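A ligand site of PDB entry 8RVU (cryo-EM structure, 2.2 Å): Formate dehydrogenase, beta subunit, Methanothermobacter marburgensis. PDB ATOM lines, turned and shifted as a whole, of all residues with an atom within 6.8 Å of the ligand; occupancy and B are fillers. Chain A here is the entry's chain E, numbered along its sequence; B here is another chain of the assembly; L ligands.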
ATOM      1  N   TRP A 277      -0.208 -19.477  12.916  1.00  0.00           N
ATOM      2  CA  TRP A 277       1.016 -18.751  12.597  1.00  0.00           C
ATOM      3  C   TRP A 277       0.868 -17.948  11.315  1.00  0.00           C
ATOM      4  O   TRP A 277       1.531 -16.916  11.147  1.00  0.00           O
ATOM      5  CB  TRP A 277       2.197 -19.716  12.472  1.00  0.00           C
ATOM      6  CG  TRP A 277       2.522 -20.489  13.723  1.00  0.00           C
ATOM      7  CD1 TRP A 277       2.777 -21.830  13.811  1.00  0.00           C
ATOM      8  CD2 TRP A 277       2.618 -19.985  15.064  1.00  0.00           C
ATOM      9  NE1 TRP A 277       3.029 -22.182  15.123  1.00  0.00           N
ATOM     10  CE2 TRP A 277       2.936 -21.073  15.911  1.00  0.00           C
ATOM     11  CE3 TRP A 277       2.475 -18.711  15.630  1.00  0.00           C
ATOM     12  CZ2 TRP A 277       3.118 -20.923  17.278  1.00  0.00           C
ATOM     13  CZ3 TRP A 277       2.643 -18.568  16.992  1.00  0.00           C
ATOM     14  CH2 TRP A 277       2.963 -19.671  17.800  1.00  0.00           C
ATOM     15  N   ARG A 279      -1.360 -16.047  10.630  1.00  0.00           N
ATOM     16  CA  ARG A 279      -1.979 -14.767  10.948  1.00  0.00           C
ATOM     17  C   ARG A 279      -0.975 -13.716  11.390  1.00  0.00           C
ATOM     18  O   ARG A 279      -1.200 -12.521  11.155  1.00  0.00           O
ATOM     19  CB  ARG A 279      -3.011 -14.949  12.064  1.00  0.00           C
ATOM     20  CG  ARG A 279      -4.371 -15.443  11.609  1.00  0.00           C
ATOM     21  CD  ARG A 279      -5.375 -15.293  12.731  1.00  0.00           C
ATOM     22  NE  ARG A 279      -6.336 -16.384  12.777  1.00  0.00           N
ATOM     23  CZ  ARG A 279      -7.010 -16.747  13.856  1.00  0.00           C
ATOM     24  NH1 ARG A 279      -6.847 -16.133  15.020  1.00  0.00           N
ATOM     25  NH2 ARG A 279      -7.859 -17.764  13.776  1.00  0.00           N
ATOM     26  N   CYS A 280       0.110 -14.132  12.040  1.00  0.00           N
ATOM     27  CA  CYS A 280       0.962 -13.208  12.784  1.00  0.00           C
ATOM     28  C   CYS A 280       1.350 -11.998  11.928  1.00  0.00           C
ATOM     29  O   CYS A 280       1.790 -12.144  10.789  1.00  0.00           O
ATOM     30  CB  CYS A 280       2.215 -13.931  13.276  1.00  0.00           C
ATOM     31  SG  CYS A 280       3.410 -12.878  14.113  1.00  0.00           S
ATOM     32  N   ILE A 281       1.185 -10.805  12.509  1.00  0.00           N
ATOM     33  CA  ILE A 281       1.505  -9.561  11.827  1.00  0.00           C
ATOM     34  C   ILE A 281       2.839  -8.993  12.289  1.00  0.00           C
ATOM     35  O   ILE A 281       3.180  -7.862  11.922  1.00  0.00           O
ATOM     36  CB  ILE A 281       0.374  -8.530  12.001  1.00  0.00           C
ATOM     37  CG1 ILE A 281       0.025  -8.359  13.486  1.00  0.00           C
ATOM     38  CG2 ILE A 281      -0.852  -8.941  11.209  1.00  0.00           C
ATOM     39  CD1 ILE A 281      -0.424  -6.966  13.839  1.00  0.00           C
ATOM     40  N   ASN A 282       3.611  -9.741  13.078  1.00  0.00           N
ATOM     41  CA  ASN A 282       4.957  -9.338  13.475  1.00  0.00           C
ATOM     42  C   ASN A 282       4.936  -8.022  14.242  1.00  0.00           C
ATOM     43  O   ASN A 282       5.804  -7.162  14.063  1.00  0.00           O
ATOM     44  CB  ASN A 282       5.864  -9.243  12.251  1.00  0.00           C
ATOM     45  CG  ASN A 282       7.322  -9.482  12.586  1.00  0.00           C
ATOM     46  OD1 ASN A 282       7.660 -10.440  13.295  1.00  0.00           O
ATOM     47  ND2 ASN A 282       8.196  -8.633  12.075  1.00  0.00           N
ATOM     48  N   CYS A 283       3.931  -7.853  15.109  1.00  0.00           N
ATOM     49  CA  CYS A 283       3.780  -6.618  15.873  1.00  0.00           C
ATOM     50  C   CYS A 283       4.584  -6.611  17.166  1.00  0.00           C
ATOM     51  O   CYS A 283       4.758  -5.541  17.752  1.00  0.00           O
ATOM     52  CB  CYS A 283       2.302  -6.385  16.187  1.00  0.00           C
ATOM     53  SG  CYS A 283       1.625  -7.508  17.423  1.00  0.00           S
ATOM     54  N   PHE A 284       5.058  -7.766  17.632  1.00  0.00           N
ATOM     55  CA  PHE A 284       5.866  -7.889  18.837  1.00  0.00           C
ATOM     56  C   PHE A 284       5.102  -7.510  20.101  1.00  0.00           C
ATOM     57  O   PHE A 284       5.722  -7.177  21.125  1.00  0.00           O
ATOM     58  CB  PHE A 284       7.152  -7.043  18.742  1.00  0.00           C
ATOM     59  CG  PHE A 284       8.142  -7.581  17.765  1.00  0.00           C
ATOM     60  CD1 PHE A 284       9.024  -8.578  18.131  1.00  0.00           C
ATOM     61  CD2 PHE A 284       8.201  -7.084  16.475  1.00  0.00           C
ATOM     62  CE1 PHE A 284       9.947  -9.078  17.239  1.00  0.00           C
ATOM     63  CE2 PHE A 284       9.119  -7.583  15.573  1.00  0.00           C
ATOM     64  CZ  PHE A 284       9.988  -8.580  15.958  1.00  0.00           C
ATOM     65  N   ALA A 285       3.771  -7.552  20.071  1.00  0.00           N
ATOM     66  CA  ALA A 285       3.010  -7.279  21.287  1.00  0.00           C
ATOM     67  C   ALA A 285       3.277  -8.331  22.346  1.00  0.00           C
ATOM     68  O   ALA A 285       3.377  -8.019  23.540  1.00  0.00           O
ATOM     69  CB  ALA A 285       1.513  -7.211  20.966  1.00  0.00           C
ATOM     70  N   CYS A 286       3.407  -9.596  21.934  1.00  0.00           N
ATOM     71  CA  CYS A 286       3.671 -10.671  22.876  1.00  0.00           C
ATOM     72  C   CYS A 286       5.009 -10.458  23.583  1.00  0.00           C
ATOM     73  O   CYS A 286       5.102 -10.579  24.808  1.00  0.00           O
ATOM     74  CB  CYS A 286       3.647 -12.019  22.158  1.00  0.00           C
ATOM     75  SG  CYS A 286       4.493 -12.019  20.546  1.00  0.00           S
ATOM     76  N   ARG A 287       6.054 -10.137  22.818  1.00  0.00           N
ATOM     77  CA  ARG A 287       7.365  -9.925  23.424  1.00  0.00           C
ATOM     78  C   ARG A 287       7.355  -8.706  24.344  1.00  0.00           C
ATOM     79  O   ARG A 287       7.925  -8.734  25.435  1.00  0.00           O
ATOM     80  CB  ARG A 287       8.433  -9.774  22.340  1.00  0.00           C
ATOM     81  CG  ARG A 287       9.847  -9.721  22.885  1.00  0.00           C
ATOM     82  CD  ARG A 287      10.699  -8.669  22.205  1.00  0.00           C
ATOM     83  NE  ARG A 287      10.050  -7.362  22.114  1.00  0.00           N
ATOM     84  CZ  ARG A 287      10.267  -6.487  21.139  1.00  0.00           C
ATOM     85  NH1 ARG A 287      11.131  -6.722  20.176  1.00  0.00           N
ATOM     86  NH2 ARG A 287       9.585  -5.342  21.140  1.00  0.00           N
ATOM     87  N   PRO A 313       5.488 -13.901   9.659  1.00  0.00           N
ATOM     88  CA  PRO A 313       6.865 -14.393   9.795  1.00  0.00           C
ATOM     89  C   PRO A 313       6.908 -15.904   9.932  1.00  0.00           C
ATOM     90  O   PRO A 313       5.938 -16.557  10.329  1.00  0.00           O
ATOM     91  CB  PRO A 313       7.354 -13.712  11.071  1.00  0.00           C
ATOM     92  CG  PRO A 313       6.131 -13.468  11.866  1.00  0.00           C
ATOM     93  CD  PRO A 313       5.044 -13.182  10.861  1.00  0.00           C
ATOM     94  N   PHE A 318      11.048 -16.599  14.870  1.00  0.00           N
ATOM     95  CA  PHE A 318      10.447 -15.697  15.837  1.00  0.00           C
ATOM     96  C   PHE A 318      10.080 -16.413  17.121  1.00  0.00           C
ATOM     97  O   PHE A 318      10.675 -16.185  18.178  1.00  0.00           O
ATOM     98  CB  PHE A 318       9.213 -15.044  15.186  1.00  0.00           C
ATOM     99  CG  PHE A 318       8.568 -13.961  16.012  1.00  0.00           C
ATOM    100  CD1 PHE A 318       7.870 -14.261  17.171  1.00  0.00           C
ATOM    101  CD2 PHE A 318       8.634 -12.639  15.601  1.00  0.00           C
ATOM    102  CE1 PHE A 318       7.281 -13.266  17.917  1.00  0.00           C
ATOM    103  CE2 PHE A 318       8.042 -11.632  16.340  1.00  0.00           C
ATOM    104  CZ  PHE A 318       7.355 -11.954  17.501  1.00  0.00           C
ATOM    105  N   GLN A 319       9.161 -17.387  17.028  1.00  0.00           N
ATOM    106  CA  GLN A 319       8.674 -18.061  18.219  1.00  0.00           C
ATOM    107  C   GLN A 319       9.713 -19.027  18.768  1.00  0.00           C
ATOM    108  O   GLN A 319       9.919 -19.092  19.986  1.00  0.00           O
ATOM    109  CB  GLN A 319       7.371 -18.802  17.918  1.00  0.00           C
ATOM    110  CG  GLN A 319       6.291 -17.929  17.278  1.00  0.00           C
ATOM    111  CD  GLN A 319       5.671 -16.945  18.261  1.00  0.00           C
ATOM    112  OE1 GLN A 319       5.821 -17.082  19.467  1.00  0.00           O
ATOM    113  NE2 GLN A 319       4.975 -15.951  17.728  1.00  0.00           N
ATOM    114  N   CYS A 336       1.225 -12.447  26.931  1.00  0.00           N
ATOM    115  CA  CYS A 336       1.473 -12.507  25.496  1.00  0.00           C
ATOM    116  C   CYS A 336       0.199 -12.875  24.736  1.00  0.00           C
ATOM    117  O   CYS A 336      -0.104 -12.270  23.695  1.00  0.00           O
ATOM    118  CB  CYS A 336       2.570 -13.526  25.206  1.00  0.00           C
ATOM    119  SG  CYS A 336       2.322 -15.135  25.997  1.00  0.00           S
ATOM    120  N   VAL A 339      -2.401  -9.860  24.813  1.00  0.00           N
ATOM    121  CA  VAL A 339      -2.188  -8.670  23.989  1.00  0.00           C
ATOM    122  C   VAL A 339      -2.105  -8.985  22.505  1.00  0.00           C
ATOM    123  O   VAL A 339      -1.962  -8.052  21.691  1.00  0.00           O
ATOM    124  CB  VAL A 339      -0.905  -7.935  24.410  1.00  0.00           C
ATOM    125  CG1 VAL A 339      -0.979  -7.526  25.876  1.00  0.00           C
ATOM    126  CG2 VAL A 339       0.330  -8.784  24.150  1.00  0.00           C
ATOM    127  N   CYS A 340      -2.193 -10.250  22.105  1.00  0.00           N
ATOM    128  CA  CYS A 340      -1.971 -10.599  20.707  1.00  0.00           C
ATOM    129  C   CYS A 340      -3.097 -10.051  19.835  1.00  0.00           C
ATOM    130  O   CYS A 340      -4.262 -10.414  20.062  1.00  0.00           O
ATOM    131  CB  CYS A 340      -1.862 -12.114  20.542  1.00  0.00           C
ATOM    132  SG  CYS A 340      -1.546 -12.634  18.836  1.00  0.00           S
ATOM    133  N   PRO A 341      -2.818  -9.212  18.834  1.00  0.00           N
ATOM    134  CA  PRO A 341      -3.896  -8.704  17.977  1.00  0.00           C
ATOM    135  C   PRO A 341      -4.519  -9.772  17.082  1.00  0.00           C
ATOM    136  O   PRO A 341      -5.648  -9.574  16.629  1.00  0.00           O
ATOM    137  CB  PRO A 341      -3.211  -7.622  17.133  1.00  0.00           C
ATOM    138  CG  PRO A 341      -1.831  -7.470  17.660  1.00  0.00           C
ATOM    139  CD  PRO A 341      -1.498  -8.701  18.423  1.00  0.00           C
ATOM    140  N   MET A 342      -3.829 -10.877  16.816  1.00  0.00           N
ATOM    141  CA  MET A 342      -4.323 -11.900  15.905  1.00  0.00           C
ATOM    142  C   MET A 342      -4.971 -13.072  16.633  1.00  0.00           C
ATOM    143  O   MET A 342      -5.406 -14.019  15.970  1.00  0.00           O
ATOM    144  CB  MET A 342      -3.176 -12.415  15.018  1.00  0.00           C
ATOM    145  CG  MET A 342      -2.856 -11.530  13.817  1.00  0.00           C
ATOM    146  SD  MET A 342      -4.287 -10.993  12.848  1.00  0.00           S
ATOM    147  CE  MET A 342      -4.235  -9.222  13.120  1.00  0.00           C
ATOM    148  N   ASP A 343      -5.053 -13.028  17.953  1.00  0.00           N
ATOM    149  CA  ASP A 343      -5.719 -14.073  18.739  1.00  0.00           C
ATOM    150  C   ASP A 343      -5.054 -15.439  18.528  1.00  0.00           C
ATOM    151  O   ASP A 343      -5.695 -16.418  18.135  1.00  0.00           O
ATOM    152  CB  ASP A 343      -7.208 -14.128  18.409  1.00  0.00           C
ATOM    153  CG  ASP A 343      -7.952 -12.887  18.843  1.00  0.00           C
ATOM    154  OD1 ASP A 343      -8.115 -12.672  20.060  1.00  0.00           O
ATOM    155  OD2 ASP A 343      -8.380 -12.113  17.955  1.00  0.00           O
ATOM    156  N   ILE A 344      -3.756 -15.487  18.779  1.00  0.00           N
ATOM    157  CA  ILE A 344      -2.978 -16.718  18.713  1.00  0.00           C
ATOM    158  C   ILE A 344      -2.750 -17.227  20.137  1.00  0.00           C
ATOM    159  O   ILE A 344      -2.419 -16.421  21.019  1.00  0.00           O
ATOM    160  CB  ILE A 344      -1.626 -16.492  17.998  1.00  0.00           C
ATOM    161  CG1 ILE A 344      -1.865 -16.029  16.558  1.00  0.00           C
ATOM    162  CG2 ILE A 344      -0.800 -17.763  18.014  1.00  0.00           C
ATOM    163  CD1 ILE A 344      -0.640 -15.406  15.911  1.00  0.00           C
ATOM    164  N   ILE A 346      -0.426 -18.285  22.227  1.00  0.00           N
ATOM    165  CA  ILE A 346       1.024 -18.404  22.390  1.00  0.00           C
ATOM    166  C   ILE A 346       1.375 -19.033  23.741  1.00  0.00           C
ATOM    167  O   ILE A 346       2.272 -19.888  23.840  1.00  0.00           O
ATOM    168  CB  ILE A 346       1.678 -17.015  22.239  1.00  0.00           C
ATOM    169  CG1 ILE A 346       1.161 -16.285  20.988  1.00  0.00           C
ATOM    170  CG2 ILE A 346       3.181 -17.129  22.187  1.00  0.00           C
ATOM    171  CD1 ILE A 346       1.310 -14.775  21.066  1.00  0.00           C
ATOM    172  N   THR B  42      -2.831  -4.089  20.574  1.00  0.00           N
ATOM    173  CA  THR B  42      -2.362  -3.032  19.702  1.00  0.00           C
ATOM    174  C   THR B  42      -1.299  -3.566  18.760  1.00  0.00           C
ATOM    175  O   THR B  42      -0.597  -4.537  19.070  1.00  0.00           O
ATOM    176  CB  THR B  42      -1.766  -1.853  20.499  1.00  0.00           C
ATOM    177  OG1 THR B  42      -0.905  -2.355  21.528  1.00  0.00           O
ATOM    178  CG2 THR B  42      -2.869  -1.029  21.131  1.00  0.00           C
ATOM    179  N   ARG B  47       1.747   0.834  20.306  1.00  0.00           N
ATOM    180  CA  ARG B  47       2.677   0.798  21.429  1.00  0.00           C
ATOM    181  C   ARG B  47       3.808   1.818  21.287  1.00  0.00           C
ATOM    182  O   ARG B  47       4.493   2.096  22.268  1.00  0.00           O
ATOM    183  CB  ARG B  47       3.255  -0.610  21.575  1.00  0.00           C
ATOM    184  CG  ARG B  47       2.498  -1.470  22.581  1.00  0.00           C
ATOM    185  CD  ARG B  47       2.783  -2.949  22.409  1.00  0.00           C
ATOM    186  NE  ARG B  47       2.188  -3.490  21.192  1.00  0.00           N
ATOM    187  CZ  ARG B  47       2.863  -3.962  20.151  1.00  0.00           C
ATOM    188  NH1 ARG B  47       4.187  -3.972  20.128  1.00  0.00           N
ATOM    189  NH2 ARG B  47       2.189  -4.447  19.107  1.00  0.00           N
HETATM  190 FE1  LIG L   1       0.510 -12.034  17.999  1.00  0.00          FE
HETATM  191 FE2  LIG L   1       3.147 -11.778  18.695  1.00  0.00          FE
HETATM  192 FE3  LIG L   1       1.898  -9.791  17.302  1.00  0.00          FE
HETATM  193 FE4  LIG L   1       2.455 -12.170  16.081  1.00  0.00          FE
HETATM  194  S1  LIG L   1       3.960 -10.658  16.888  1.00  0.00           S
HETATM  195  S2  LIG L   1       0.497 -11.003  15.973  1.00  0.00           S
HETATM  196  S3  LIG L   1       2.135 -13.627  17.807  1.00  0.00           S
HETATM  197  S4  LIG L   1       1.408 -10.494  19.412  1.00  0.00           S
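Asn 282 touches the ligand (CA to S1, 3.8 Å). Ala 285 touches the ligand. Phe 318 touches the ligand (CZ to S1, 3.7 Å). Pro 341 touches the ligand (CD to S4, 3.6 Å). Ile 344 touches the ligand (CD1 to S3, 3.8 Å). CD1 of Ile 346 touches S3 of the ligand, 3.6 Å away. Of the 23 residues printed, 13 come within 4 Å of the ligand.
The side-chain sulfur (SG) of Cys 280 sits close to the backbone NH (N) of Asn 282, at 3.3 Å. The backbone NH of Ala 285 lies close to the side-chain sulfur of Cys 283 (3.4 Å). The guanidinium group (NH1) of Arg 47 of chain B lies within hydrogen-bond range of the backbone carbonyl oxygen (O) of Cys 283, at 2.9 Å. The backbone NH (N) of Met 342 lies close to the side-chain sulfur (SG) of Cys 340, at 3.5 Å. SG of Cys 340 sits close to N of Asp 343, at 3.6 Å. SG of Cys 340 sits close to N of Ile 344 (3.6 Å).
NE2 of Gln 319 sits close to S3 of the ligand, 3.7 Å away. The side-chain sulfur (SG) of Cys 340 is bound to an iron atom (FE1) of the ligand, 2.3 Å away. An iron atom (FE2) of the ligand is bound by the side-chain sulfur (SG) of Cys 286, 2.3 Å away. S1 of the ligand sits close to N of Phe 284 (3.2 Å). The backbone NH (N) of Ile 281 sits close to a sulfur (S2) of the ligand. A sulfur (S1) of the ligand lies close to the backbone NH of Cys 283. The side-chain sulfur (SG) of Cys 283 binds an iron atom (FE3) of the ligand, at 2.3 Å. A sulfur (S4) of the ligand sits close to the backbone NH (N) of Cys 286. The side-chain sulfur (SG) of Cys 280 binds an iron atom (FE4) of the ligand, at 2.3 Å.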
